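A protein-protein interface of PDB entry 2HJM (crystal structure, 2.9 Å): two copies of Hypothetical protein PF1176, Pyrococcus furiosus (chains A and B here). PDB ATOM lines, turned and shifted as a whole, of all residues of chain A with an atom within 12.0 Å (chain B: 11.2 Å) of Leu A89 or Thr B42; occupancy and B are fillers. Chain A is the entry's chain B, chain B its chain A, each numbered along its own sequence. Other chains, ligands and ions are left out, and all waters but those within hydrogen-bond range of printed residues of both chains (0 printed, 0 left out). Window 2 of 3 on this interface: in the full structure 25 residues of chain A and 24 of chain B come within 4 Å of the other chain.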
ATOM      1  N   ARG A  43       2.865  23.955 -21.897  1.00  0.00           N
ATOM      2  CA  ARG A  43       2.331  22.980 -22.851  1.00  0.00           C
ATOM      3  C   ARG A  43       1.330  23.572 -23.826  1.00  0.00           C
ATOM      4  O   ARG A  43       0.838  22.888 -24.728  1.00  0.00           O
ATOM      5  CB  ARG A  43       1.646  21.828 -22.112  1.00  0.00           C
ATOM      6  CG  ARG A  43       2.542  20.970 -21.259  1.00  0.00           C
ATOM      7  CD  ARG A  43       3.367  20.025 -22.084  1.00  0.00           C
ATOM      8  NE  ARG A  43       4.113  19.141 -21.197  1.00  0.00           N
ATOM      9  CZ  ARG A  43       4.997  18.236 -21.597  1.00  0.00           C
ATOM     10  NH1 ARG A  43       5.254  18.081 -22.884  1.00  0.00           N
ATOM     11  NH2 ARG A  43       5.638  17.502 -20.699  1.00  0.00           N
ATOM     12  N   GLY A  44       1.001  24.837 -23.645  1.00  0.00           N
ATOM     13  CA  GLY A  44       0.042  25.426 -24.548  1.00  0.00           C
ATOM     14  C   GLY A  44      -1.313  25.535 -23.898  1.00  0.00           C
ATOM     15  O   GLY A  44      -1.532  25.059 -22.793  1.00  0.00           O
ATOM     16  N   GLU A  45      -2.235  26.160 -24.606  1.00  0.00           N
ATOM     17  CA  GLU A  45      -3.568  26.376 -24.100  1.00  0.00           C
ATOM     18  C   GLU A  45      -4.434  25.149 -24.280  1.00  0.00           C
ATOM     19  O   GLU A  45      -5.209  24.796 -23.394  1.00  0.00           O
ATOM     20  CB  GLU A  45      -4.174  27.570 -24.822  1.00  0.00           C
ATOM     21  CG  GLU A  45      -5.455  28.076 -24.262  1.00  0.00           C
ATOM     22  CD  GLU A  45      -5.827  29.411 -24.854  1.00  0.00           C
ATOM     23  OE1 GLU A  45      -6.938  29.897 -24.559  1.00  0.00           O
ATOM     24  OE2 GLU A  45      -5.004  29.979 -25.611  1.00  0.00           O
ATOM     25  N   ALA A  46      -4.305  24.490 -25.424  1.00  0.00           N
ATOM     26  CA  ALA A  46      -5.107  23.308 -25.679  1.00  0.00           C
ATOM     27  C   ALA A  46      -4.843  22.279 -24.584  1.00  0.00           C
ATOM     28  O   ALA A  46      -5.767  21.627 -24.095  1.00  0.00           O
ATOM     29  CB  ALA A  46      -4.774  22.740 -27.031  1.00  0.00           C
ATOM     30  N   PHE A  47      -3.581  22.162 -24.189  1.00  0.00           N
ATOM     31  CA  PHE A  47      -3.183  21.231 -23.149  1.00  0.00           C
ATOM     32  C   PHE A  47      -3.856  21.534 -21.813  1.00  0.00           C
ATOM     33  O   PHE A  47      -4.500  20.679 -21.224  1.00  0.00           O
ATOM     34  CB  PHE A  47      -1.667  21.285 -22.975  1.00  0.00           C
ATOM     35  CG  PHE A  47      -1.099  20.114 -22.220  1.00  0.00           C
ATOM     36  CD1 PHE A  47      -1.269  20.002 -20.842  1.00  0.00           C
ATOM     37  CD2 PHE A  47      -0.396  19.120 -22.893  1.00  0.00           C
ATOM     38  CE1 PHE A  47      -0.746  18.917 -20.151  1.00  0.00           C
ATOM     39  CE2 PHE A  47       0.124  18.040 -22.210  1.00  0.00           C
ATOM     40  CZ  PHE A  47      -0.050  17.939 -20.836  1.00  0.00           C
ATOM     41  N   ALA A  50      -7.540  20.742 -21.842  1.00  0.00           N
ATOM     42  CA  ALA A  50      -7.868  19.325 -21.914  1.00  0.00           C
ATOM     43  C   ALA A  50      -7.764  18.637 -20.551  1.00  0.00           C
ATOM     44  O   ALA A  50      -8.524  17.714 -20.266  1.00  0.00           O
ATOM     45  CB  ALA A  50      -6.964  18.626 -22.928  1.00  0.00           C
ATOM     46  N   THR A  81     -18.323  18.963 -25.213  1.00  0.00           N
ATOM     47  CA  THR A  81     -18.203  19.774 -26.408  1.00  0.00           C
ATOM     48  C   THR A  81     -16.902  20.552 -26.358  1.00  0.00           C
ATOM     49  O   THR A  81     -16.114  20.552 -27.316  1.00  0.00           O
ATOM     50  CB  THR A  81     -19.358  20.779 -26.498  1.00  0.00           C
ATOM     51  OG1 THR A  81     -20.602  20.075 -26.460  1.00  0.00           O
ATOM     52  CG2 THR A  81     -19.272  21.579 -27.782  1.00  0.00           C
ATOM     53  N   ALA A  82     -16.695  21.216 -25.225  1.00  0.00           N
ATOM     54  CA  ALA A  82     -15.512  22.026 -24.997  1.00  0.00           C
ATOM     55  C   ALA A  82     -14.248  21.256 -25.337  1.00  0.00           C
ATOM     56  O   ALA A  82     -13.321  21.791 -25.936  1.00  0.00           O
ATOM     57  CB  ALA A  82     -15.477  22.467 -23.550  1.00  0.00           C
ATOM     58  N   ARG A  83     -14.229  19.988 -24.948  1.00  0.00           N
ATOM     59  CA  ARG A  83     -13.085  19.130 -25.191  1.00  0.00           C
ATOM     60  C   ARG A  83     -12.939  18.792 -26.651  1.00  0.00           C
ATOM     61  O   ARG A  83     -11.879  18.993 -27.239  1.00  0.00           O
ATOM     62  CB  ARG A  83     -13.210  17.855 -24.370  1.00  0.00           C
ATOM     63  CG  ARG A  83     -12.973  18.088 -22.889  1.00  0.00           C
ATOM     64  CD  ARG A  83     -13.160  16.819 -22.077  1.00  0.00           C
ATOM     65  NE  ARG A  83     -12.452  15.691 -22.679  1.00  0.00           N
ATOM     66  CZ  ARG A  83     -13.026  14.761 -23.436  1.00  0.00           C
ATOM     67  NH1 ARG A  83     -14.324  14.804 -23.693  1.00  0.00           N
ATOM     68  NH2 ARG A  83     -12.297  13.782 -23.935  1.00  0.00           N
ATOM     69  N   GLU A  84     -14.009  18.281 -27.239  1.00  0.00           N
ATOM     70  CA  GLU A  84     -13.978  17.918 -28.650  1.00  0.00           C
ATOM     71  C   GLU A  84     -13.358  19.060 -29.451  1.00  0.00           C
ATOM     72  O   GLU A  84     -12.510  18.838 -30.315  1.00  0.00           O
ATOM     73  CB  GLU A  84     -15.391  17.611 -29.147  1.00  0.00           C
ATOM     74  CG  GLU A  84     -16.006  16.372 -28.516  1.00  0.00           C
ATOM     75  CD  GLU A  84     -17.457  16.155 -28.931  1.00  0.00           C
ATOM     76  OE1 GLU A  84     -18.053  15.137 -28.504  1.00  0.00           O
ATOM     77  OE2 GLU A  84     -18.006  17.003 -29.682  1.00  0.00           O
ATOM     78  N   GLU A  85     -13.779  20.285 -29.148  1.00  0.00           N
ATOM     79  CA  GLU A  85     -13.247  21.461 -29.821  1.00  0.00           C
ATOM     80  C   GLU A  85     -11.782  21.658 -29.483  1.00  0.00           C
ATOM     81  O   GLU A  85     -10.961  21.839 -30.363  1.00  0.00           O
ATOM     82  CB  GLU A  85     -14.020  22.707 -29.407  1.00  0.00           C
ATOM     83  CG  GLU A  85     -13.452  23.970 -29.990  1.00  0.00           C
ATOM     84  CD  GLU A  85     -13.384  23.905 -31.492  1.00  0.00           C
ATOM     85  OE1 GLU A  85     -12.435  24.462 -32.083  1.00  0.00           O
ATOM     86  OE2 GLU A  85     -14.296  23.294 -32.084  1.00  0.00           O
ATOM     87  N   THR A  86     -11.458  21.622 -28.200  1.00  0.00           N
ATOM     88  CA  THR A  86     -10.086  21.824 -27.760  1.00  0.00           C
ATOM     89  C   THR A  86      -9.097  20.895 -28.405  1.00  0.00           C
ATOM     90  O   THR A  86      -8.080  21.338 -28.921  1.00  0.00           O
ATOM     91  CB  THR A  86      -9.945  21.669 -26.233  1.00  0.00           C
ATOM     92  OG1 THR A  86     -10.654  22.731 -25.589  1.00  0.00           O
ATOM     93  CG2 THR A  86      -8.472  21.700 -25.806  1.00  0.00           C
ATOM     94  N   GLU A  87      -9.391  19.602 -28.392  1.00  0.00           N
ATOM     95  CA  GLU A  87      -8.447  18.658 -28.965  1.00  0.00           C
ATOM     96  C   GLU A  87      -8.356  18.654 -30.491  1.00  0.00           C
ATOM     97  O   GLU A  87      -7.381  18.152 -31.034  1.00  0.00           O
ATOM     98  CB  GLU A  87      -8.681  17.240 -28.390  1.00  0.00           C
ATOM     99  CG  GLU A  87      -9.960  16.511 -28.794  1.00  0.00           C
ATOM    100  CD  GLU A  87     -10.346  15.392 -27.798  1.00  0.00           C
ATOM    101  OE1 GLU A  87     -11.132  14.484 -28.176  1.00  0.00           O
ATOM    102  OE2 GLU A  87      -9.881  15.429 -26.626  1.00  0.00           O
ATOM    103  N   ALA A  88      -9.334  19.242 -31.179  1.00  0.00           N
ATOM    104  CA  ALA A  88      -9.316  19.306 -32.646  1.00  0.00           C
ATOM    105  C   ALA A  88      -8.243  20.237 -33.195  1.00  0.00           C
ATOM    106  O   ALA A  88      -8.060  21.345 -32.721  1.00  0.00           O
ATOM    107  CB  ALA A  88     -10.659  19.751 -33.169  1.00  0.00           C
ATOM    108  N   LEU A  89      -7.534  19.787 -34.215  1.00  0.00           N
ATOM    109  CA  LEU A  89      -6.497  20.609 -34.812  1.00  0.00           C
ATOM    110  C   LEU A  89      -7.007  21.330 -36.049  1.00  0.00           C
ATOM    111  O   LEU A  89      -7.905  20.846 -36.726  1.00  0.00           O
ATOM    112  CB  LEU A  89      -5.300  19.748 -35.194  1.00  0.00           C
ATOM    113  CG  LEU A  89      -4.300  19.384 -34.102  1.00  0.00           C
ATOM    114  CD1 LEU A  89      -3.192  18.564 -34.713  1.00  0.00           C
ATOM    115  CD2 LEU A  89      -3.725  20.639 -33.482  1.00  0.00           C
ATOM    116  N   LEU A  90      -6.432  22.491 -36.340  1.00  0.00           N
ATOM    117  CA  LEU A  90      -6.820  23.255 -37.518  1.00  0.00           C
ATOM    118  C   LEU A  90      -6.324  22.556 -38.778  1.00  0.00           C
ATOM    119  O   LEU A  90      -7.022  22.518 -39.794  1.00  0.00           O
ATOM    120  CB  LEU A  90      -6.216  24.652 -37.474  1.00  0.00           C
ATOM    121  CG  LEU A  90      -6.998  25.747 -36.765  1.00  0.00           C
ATOM    122  CD1 LEU A  90      -6.250  27.070 -36.911  1.00  0.00           C
ATOM    123  CD2 LEU A  90      -8.391  25.841 -37.378  1.00  0.00           C
ATOM    124  N   ARG A  91      -5.109  22.011 -38.700  1.00  0.00           N
ATOM    125  CA  ARG A  91      -4.481  21.324 -39.829  1.00  0.00           C
ATOM    126  C   ARG A  91      -4.352  22.294 -41.018  1.00  0.00           C
ATOM    127  O   ARG A  91      -5.005  22.069 -42.073  1.00  0.00           O
ATOM    128  CB  ARG A  91      -5.301  20.082 -40.221  1.00  0.00           C
ATOM    129  N   LEU B  35     -13.067   6.635 -26.575  1.00  0.00           N
ATOM    130  CA  LEU B  35     -13.370   7.825 -27.365  1.00  0.00           C
ATOM    131  C   LEU B  35     -12.276   8.892 -27.313  1.00  0.00           C
ATOM    132  O   LEU B  35     -12.542  10.060 -27.570  1.00  0.00           O
ATOM    133  CB  LEU B  35     -14.711   8.429 -26.912  1.00  0.00           C
ATOM    134  N   THR B  36     -11.048   8.500 -26.988  1.00  0.00           N
ATOM    135  CA  THR B  36      -9.944   9.452 -26.897  1.00  0.00           C
ATOM    136  C   THR B  36      -8.635   8.827 -27.357  1.00  0.00           C
ATOM    137  O   THR B  36      -7.563   9.207 -26.892  1.00  0.00           O
ATOM    138  CB  THR B  36      -9.809   9.941 -25.457  1.00  0.00           C
ATOM    139  N   HIS B  37      -8.726   7.874 -28.281  1.00  0.00           N
ATOM    140  CA  HIS B  37      -7.550   7.161 -28.783  1.00  0.00           C
ATOM    141  C   HIS B  37      -6.736   7.926 -29.826  1.00  0.00           C
ATOM    142  O   HIS B  37      -5.496   7.910 -29.790  1.00  0.00           O
ATOM    143  CB  HIS B  37      -7.970   5.806 -29.347  1.00  0.00           C
ATOM    144  N   GLY B  38      -7.429   8.584 -30.752  1.00  0.00           N
ATOM    145  CA  GLY B  38      -6.749   9.341 -31.794  1.00  0.00           C
ATOM    146  C   GLY B  38      -5.950  10.533 -31.293  1.00  0.00           C
ATOM    147  O   GLY B  38      -4.951  10.898 -31.907  1.00  0.00           O
ATOM    148  N   ILE B  39      -6.389  11.129 -30.182  1.00  0.00           N
ATOM    149  CA  ILE B  39      -5.727  12.290 -29.586  1.00  0.00           C
ATOM    150  C   ILE B  39      -4.213  12.140 -29.623  1.00  0.00           C
ATOM    151  O   ILE B  39      -3.490  13.055 -30.020  1.00  0.00           O
ATOM    152  CB  ILE B  39      -6.202  12.484 -28.133  1.00  0.00           C
ATOM    153  N   GLU B  40      -3.752  10.969 -29.209  1.00  0.00           N
ATOM    154  CA  GLU B  40      -2.333  10.648 -29.165  1.00  0.00           C
ATOM    155  C   GLU B  40      -1.702  10.894 -30.525  1.00  0.00           C
ATOM    156  O   GLU B  40      -0.608  11.460 -30.642  1.00  0.00           O
ATOM    157  CB  GLU B  40      -2.177   9.180 -28.771  1.00  0.00           C
ATOM    158  CG  GLU B  40      -0.902   8.849 -28.020  1.00  0.00           C
ATOM    159  CD  GLU B  40      -1.037   7.563 -27.209  1.00  0.00           C
ATOM    160  OE1 GLU B  40      -1.842   7.534 -26.248  1.00  0.00           O
ATOM    161  OE2 GLU B  40      -0.344   6.578 -27.540  1.00  0.00           O
ATOM    162  N   LYS B  41      -2.421  10.456 -31.552  1.00  0.00           N
ATOM    163  CA  LYS B  41      -1.987  10.592 -32.934  1.00  0.00           C
ATOM    164  C   LYS B  41      -1.732  12.059 -33.275  1.00  0.00           C
ATOM    165  O   LYS B  41      -0.641  12.427 -33.723  1.00  0.00           O
ATOM    166  CB  LYS B  41      -3.056  10.006 -33.867  1.00  0.00           C
ATOM    167  N   THR B  42      -2.741  12.888 -33.025  1.00  0.00           N
ATOM    168  CA  THR B  42      -2.700  14.312 -33.313  1.00  0.00           C
ATOM    169  C   THR B  42      -2.012  15.261 -32.349  1.00  0.00           C
ATOM    170  O   THR B  42      -1.390  16.213 -32.792  1.00  0.00           O
ATOM    171  CB  THR B  42      -4.100  14.828 -33.504  1.00  0.00           C
ATOM    172  OG1 THR B  42      -4.983  14.109 -32.627  1.00  0.00           O
ATOM    173  CG2 THR B  42      -4.529  14.647 -34.940  1.00  0.00           C
ATOM    174  N   ARG B  43      -2.128  15.031 -31.043  1.00  0.00           N
ATOM    175  CA  ARG B  43      -1.509  15.938 -30.069  1.00  0.00           C
ATOM    176  C   ARG B  43      -0.352  15.316 -29.317  1.00  0.00           C
ATOM    177  O   ARG B  43       0.397  16.012 -28.622  1.00  0.00           O
ATOM    178  CB  ARG B  43      -2.531  16.402 -29.031  1.00  0.00           C
ATOM    179  CG  ARG B  43      -3.715  17.151 -29.573  1.00  0.00           C
ATOM    180  CD  ARG B  43      -3.456  18.624 -29.652  1.00  0.00           C
ATOM    181  NE  ARG B  43      -4.627  19.294 -30.198  1.00  0.00           N
ATOM    182  CZ  ARG B  43      -4.720  20.603 -30.384  1.00  0.00           C
ATOM    183  NH1 ARG B  43      -3.704  21.401 -30.056  1.00  0.00           N
ATOM    184  NH2 ARG B  43      -5.824  21.104 -30.928  1.00  0.00           N
ATOM    185  N   GLY B  44      -0.225  14.000 -29.424  1.00  0.00           N
ATOM    186  CA  GLY B  44       0.842  13.333 -28.717  1.00  0.00           C
ATOM    187  C   GLY B  44       0.401  12.607 -27.456  1.00  0.00           C
ATOM    188  O   GLY B  44      -0.775  12.565 -27.077  1.00  0.00           O
ATOM    189  N   GLU B  45       1.403  12.054 -26.794  1.00  0.00           N
ATOM    190  CA  GLU B  45       1.253  11.270 -25.587  1.00  0.00           C
ATOM    191  C   GLU B  45       0.902  12.086 -24.330  1.00  0.00           C
ATOM    192  O   GLU B  45      -0.086  11.780 -23.642  1.00  0.00           O
ATOM    193  CB  GLU B  45       2.554  10.501 -25.390  1.00  0.00           C
ATOM    194  CG  GLU B  45       2.446   9.175 -24.699  1.00  0.00           C
ATOM    195  CD  GLU B  45       3.765   8.431 -24.705  1.00  0.00           C
ATOM    196  OE1 GLU B  45       3.901   7.498 -23.890  1.00  0.00           O
ATOM    197  OE2 GLU B  45       4.655   8.774 -25.524  1.00  0.00           O
ATOM    198  N   ALA B  46       1.706  13.111 -24.029  1.00  0.00           N
ATOM    199  CA  ALA B  46       1.473  13.938 -22.843  1.00  0.00           C
ATOM    200  C   ALA B  46       0.038  14.442 -22.807  1.00  0.00           C
ATOM    201  O   ALA B  46      -0.649  14.311 -21.803  1.00  0.00           O
ATOM    202  CB  ALA B  46       2.432  15.101 -22.816  1.00  0.00           C
ATOM    203  N   PHE B  47      -0.401  15.011 -23.919  1.00  0.00           N
ATOM    204  CA  PHE B  47      -1.754  15.524 -24.075  1.00  0.00           C
ATOM    205  C   PHE B  47      -2.782  14.410 -23.836  1.00  0.00           C
ATOM    206  O   PHE B  47      -3.773  14.593 -23.133  1.00  0.00           O
ATOM    207  CB  PHE B  47      -1.898  16.081 -25.497  1.00  0.00           C
ATOM    208  CG  PHE B  47      -3.140  16.890 -25.719  1.00  0.00           C
ATOM    209  CD1 PHE B  47      -4.379  16.273 -25.853  1.00  0.00           C
ATOM    210  CD2 PHE B  47      -3.069  18.274 -25.782  1.00  0.00           C
ATOM    211  CE1 PHE B  47      -5.529  17.022 -26.045  1.00  0.00           C
ATOM    212  CE2 PHE B  47      -4.214  19.031 -25.973  1.00  0.00           C
ATOM    213  CZ  PHE B  47      -5.447  18.400 -26.106  1.00  0.00           C
ATOM    214  N   ALA B  48      -2.538  13.250 -24.432  1.00  0.00           N
ATOM    215  CA  ALA B  48      -3.443  12.121 -24.279  1.00  0.00           C
ATOM    216  C   ALA B  48      -3.500  11.725 -22.810  1.00  0.00           C
ATOM    217  O   ALA B  48      -4.583  11.537 -22.237  1.00  0.00           O
ATOM    218  CB  ALA B  48      -2.969  10.959 -25.126  1.00  0.00           C
ATOM    219  N   LYS B  49      -2.325  11.618 -22.200  1.00  0.00           N
ATOM    220  CA  LYS B  49      -2.235  11.249 -20.805  1.00  0.00           C
ATOM    221  C   LYS B  49      -2.823  12.300 -19.863  1.00  0.00           C
ATOM    222  O   LYS B  49      -3.406  11.958 -18.834  1.00  0.00           O
ATOM    223  CB  LYS B  49      -0.783  10.993 -20.446  1.00  0.00           C
ATOM    224  CG  LYS B  49      -0.263   9.650 -20.885  1.00  0.00           C
ATOM    225  CD  LYS B  49       1.185   9.527 -20.492  1.00  0.00           C
ATOM    226  CE  LYS B  49       1.633   8.093 -20.414  1.00  0.00           C
ATOM    227  NZ  LYS B  49       3.041   8.039 -19.936  1.00  0.00           N
ATOM    228  N   SER B  51      -5.307  14.226 -20.456  1.00  0.00           N
ATOM    229  CA  SER B  51      -6.762  14.204 -20.500  1.00  0.00           C
ATOM    230  C   SER B  51      -7.293  13.022 -19.686  1.00  0.00           C
ATOM    231  O   SER B  51      -8.169  13.176 -18.835  1.00  0.00           O
ATOM    232  CB  SER B  51      -7.247  14.093 -21.939  1.00  0.00           C
ATOM    233  OG  SER B  51      -6.613  15.062 -22.757  1.00  0.00           O
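Of the 17 printed residues of chain A, 7 touch a printed residue of chain B. Hydrophobic or aromatic side chains of chain A that line the printed part of chain B: Ala A46, Phe A47, Ala A50 and Leu A89. Among the printed residues, no Asp or Glu carboxylate lies within 4 Å of a Lys or Arg side-chain nitrogen of the other chain.
The guanidinium group (NH2) of Arg B43 is in hydrogen-bond range of the backbone carbonyl oxygen (O) of Thr A86. NE of Arg B43 is in hydrogen-bond range of O of Glu A87 (3.1 Å). The guanidinium group of Arg B43 lies within hydrogen-bond range of the backbone carbonyl oxygen of Ala A88 (2.9 Å).
Ala A46 touches Arg B43. Ala A46 touches Phe B47 (O to CE2, 3.6 Å). C of Ala B46 touches CE2 of Phe A47, 3.6 Å away. Phe A47 touches Phe B47. Ala A50 touches Phe B47. OG of Ser B51 touches CB of Ala A50, at 3.6 Å. Glu A87 touches Phe B47 (CB to CE1, 3.9 Å). Thr B42 touches Leu A89 (O to CD1, 3.5 Å). Leu A89 touches Arg B43 (CD2 to CZ, 3.3 Å).
Of chain B, only Thr B42 (3.5 Å) and Arg B43 (3.3 Å) come within 4 Å of Leu A89. Thr B42 touches just one residue of chain A: Leu A89 (3.5 Å). No residue of chain B comes within 4 Å of Leu A90. No residue of chain B comes within 4 Å of Arg A91. No residue of chain A comes within 4 Å of Gly B38. No residue of chain A comes within 4 Å of Lys B41. Arg B43 touches just these residues of chain A: Ala A46, Thr A86, Glu A87, Ala A88 and Leu A89. Gly B44 touches none of the printed residues of chain A. Printed residues of chain A within 4 Å of Phe B47: Ala A46 (3.6 Å), Phe A47 (3.5 Å), Ala A50 (3.5 Å) and Glu A87 (3.9 Å). Printed residues of chain B within 4 Å of Glu A87: Arg B43 (3.1 Å) and Phe B47 (3.9 Å). Printed residues of chain A within 4 Å of Ala B46: Phe A47 (3.6 Å). Glu B40 touches none of the printed residues of chain A. The nearest residue of chain B that does not touch Leu A89 is Lys B41 (6.7 Å). The nearest printed residue of chain B that does not touch Thr A86 is Phe B47 (4.5 Å).
Ala A46 touches Arg B43, but with the chains exchanged Arg A43 does not touch Ala B46 (4.1 Å). Ala A46 touches Phe B47, and with the chains exchanged Phe A47 touches Ala B46. Phe A47 touches its own counterpart, Phe B47. Of the 12 pairs that touch across the chains among the printed residues, 3 have their exchanged pair printed and touching as well.
O of Phe B47 sits at hydrogen-bond distance from OG of Ser B51, at 2.9 Å. The guanidinium group (NH2) of Arg A83 is in salt-bridge range of the side-chain carboxylate (OE2) of Glu A87, at 3.97 Å. OG1 of Thr B42 is in hydrogen-bond range of O of Ile B39. OG1 of Thr A86 is in hydrogen-bond range of O of Ala A82, 2.8 Å away. The side-chain hydroxyl (OG1) of Thr B42 sits at hydrogen-bond distance from the backbone carbonyl oxygen (O) of Gly B38, 3.3 Å away.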
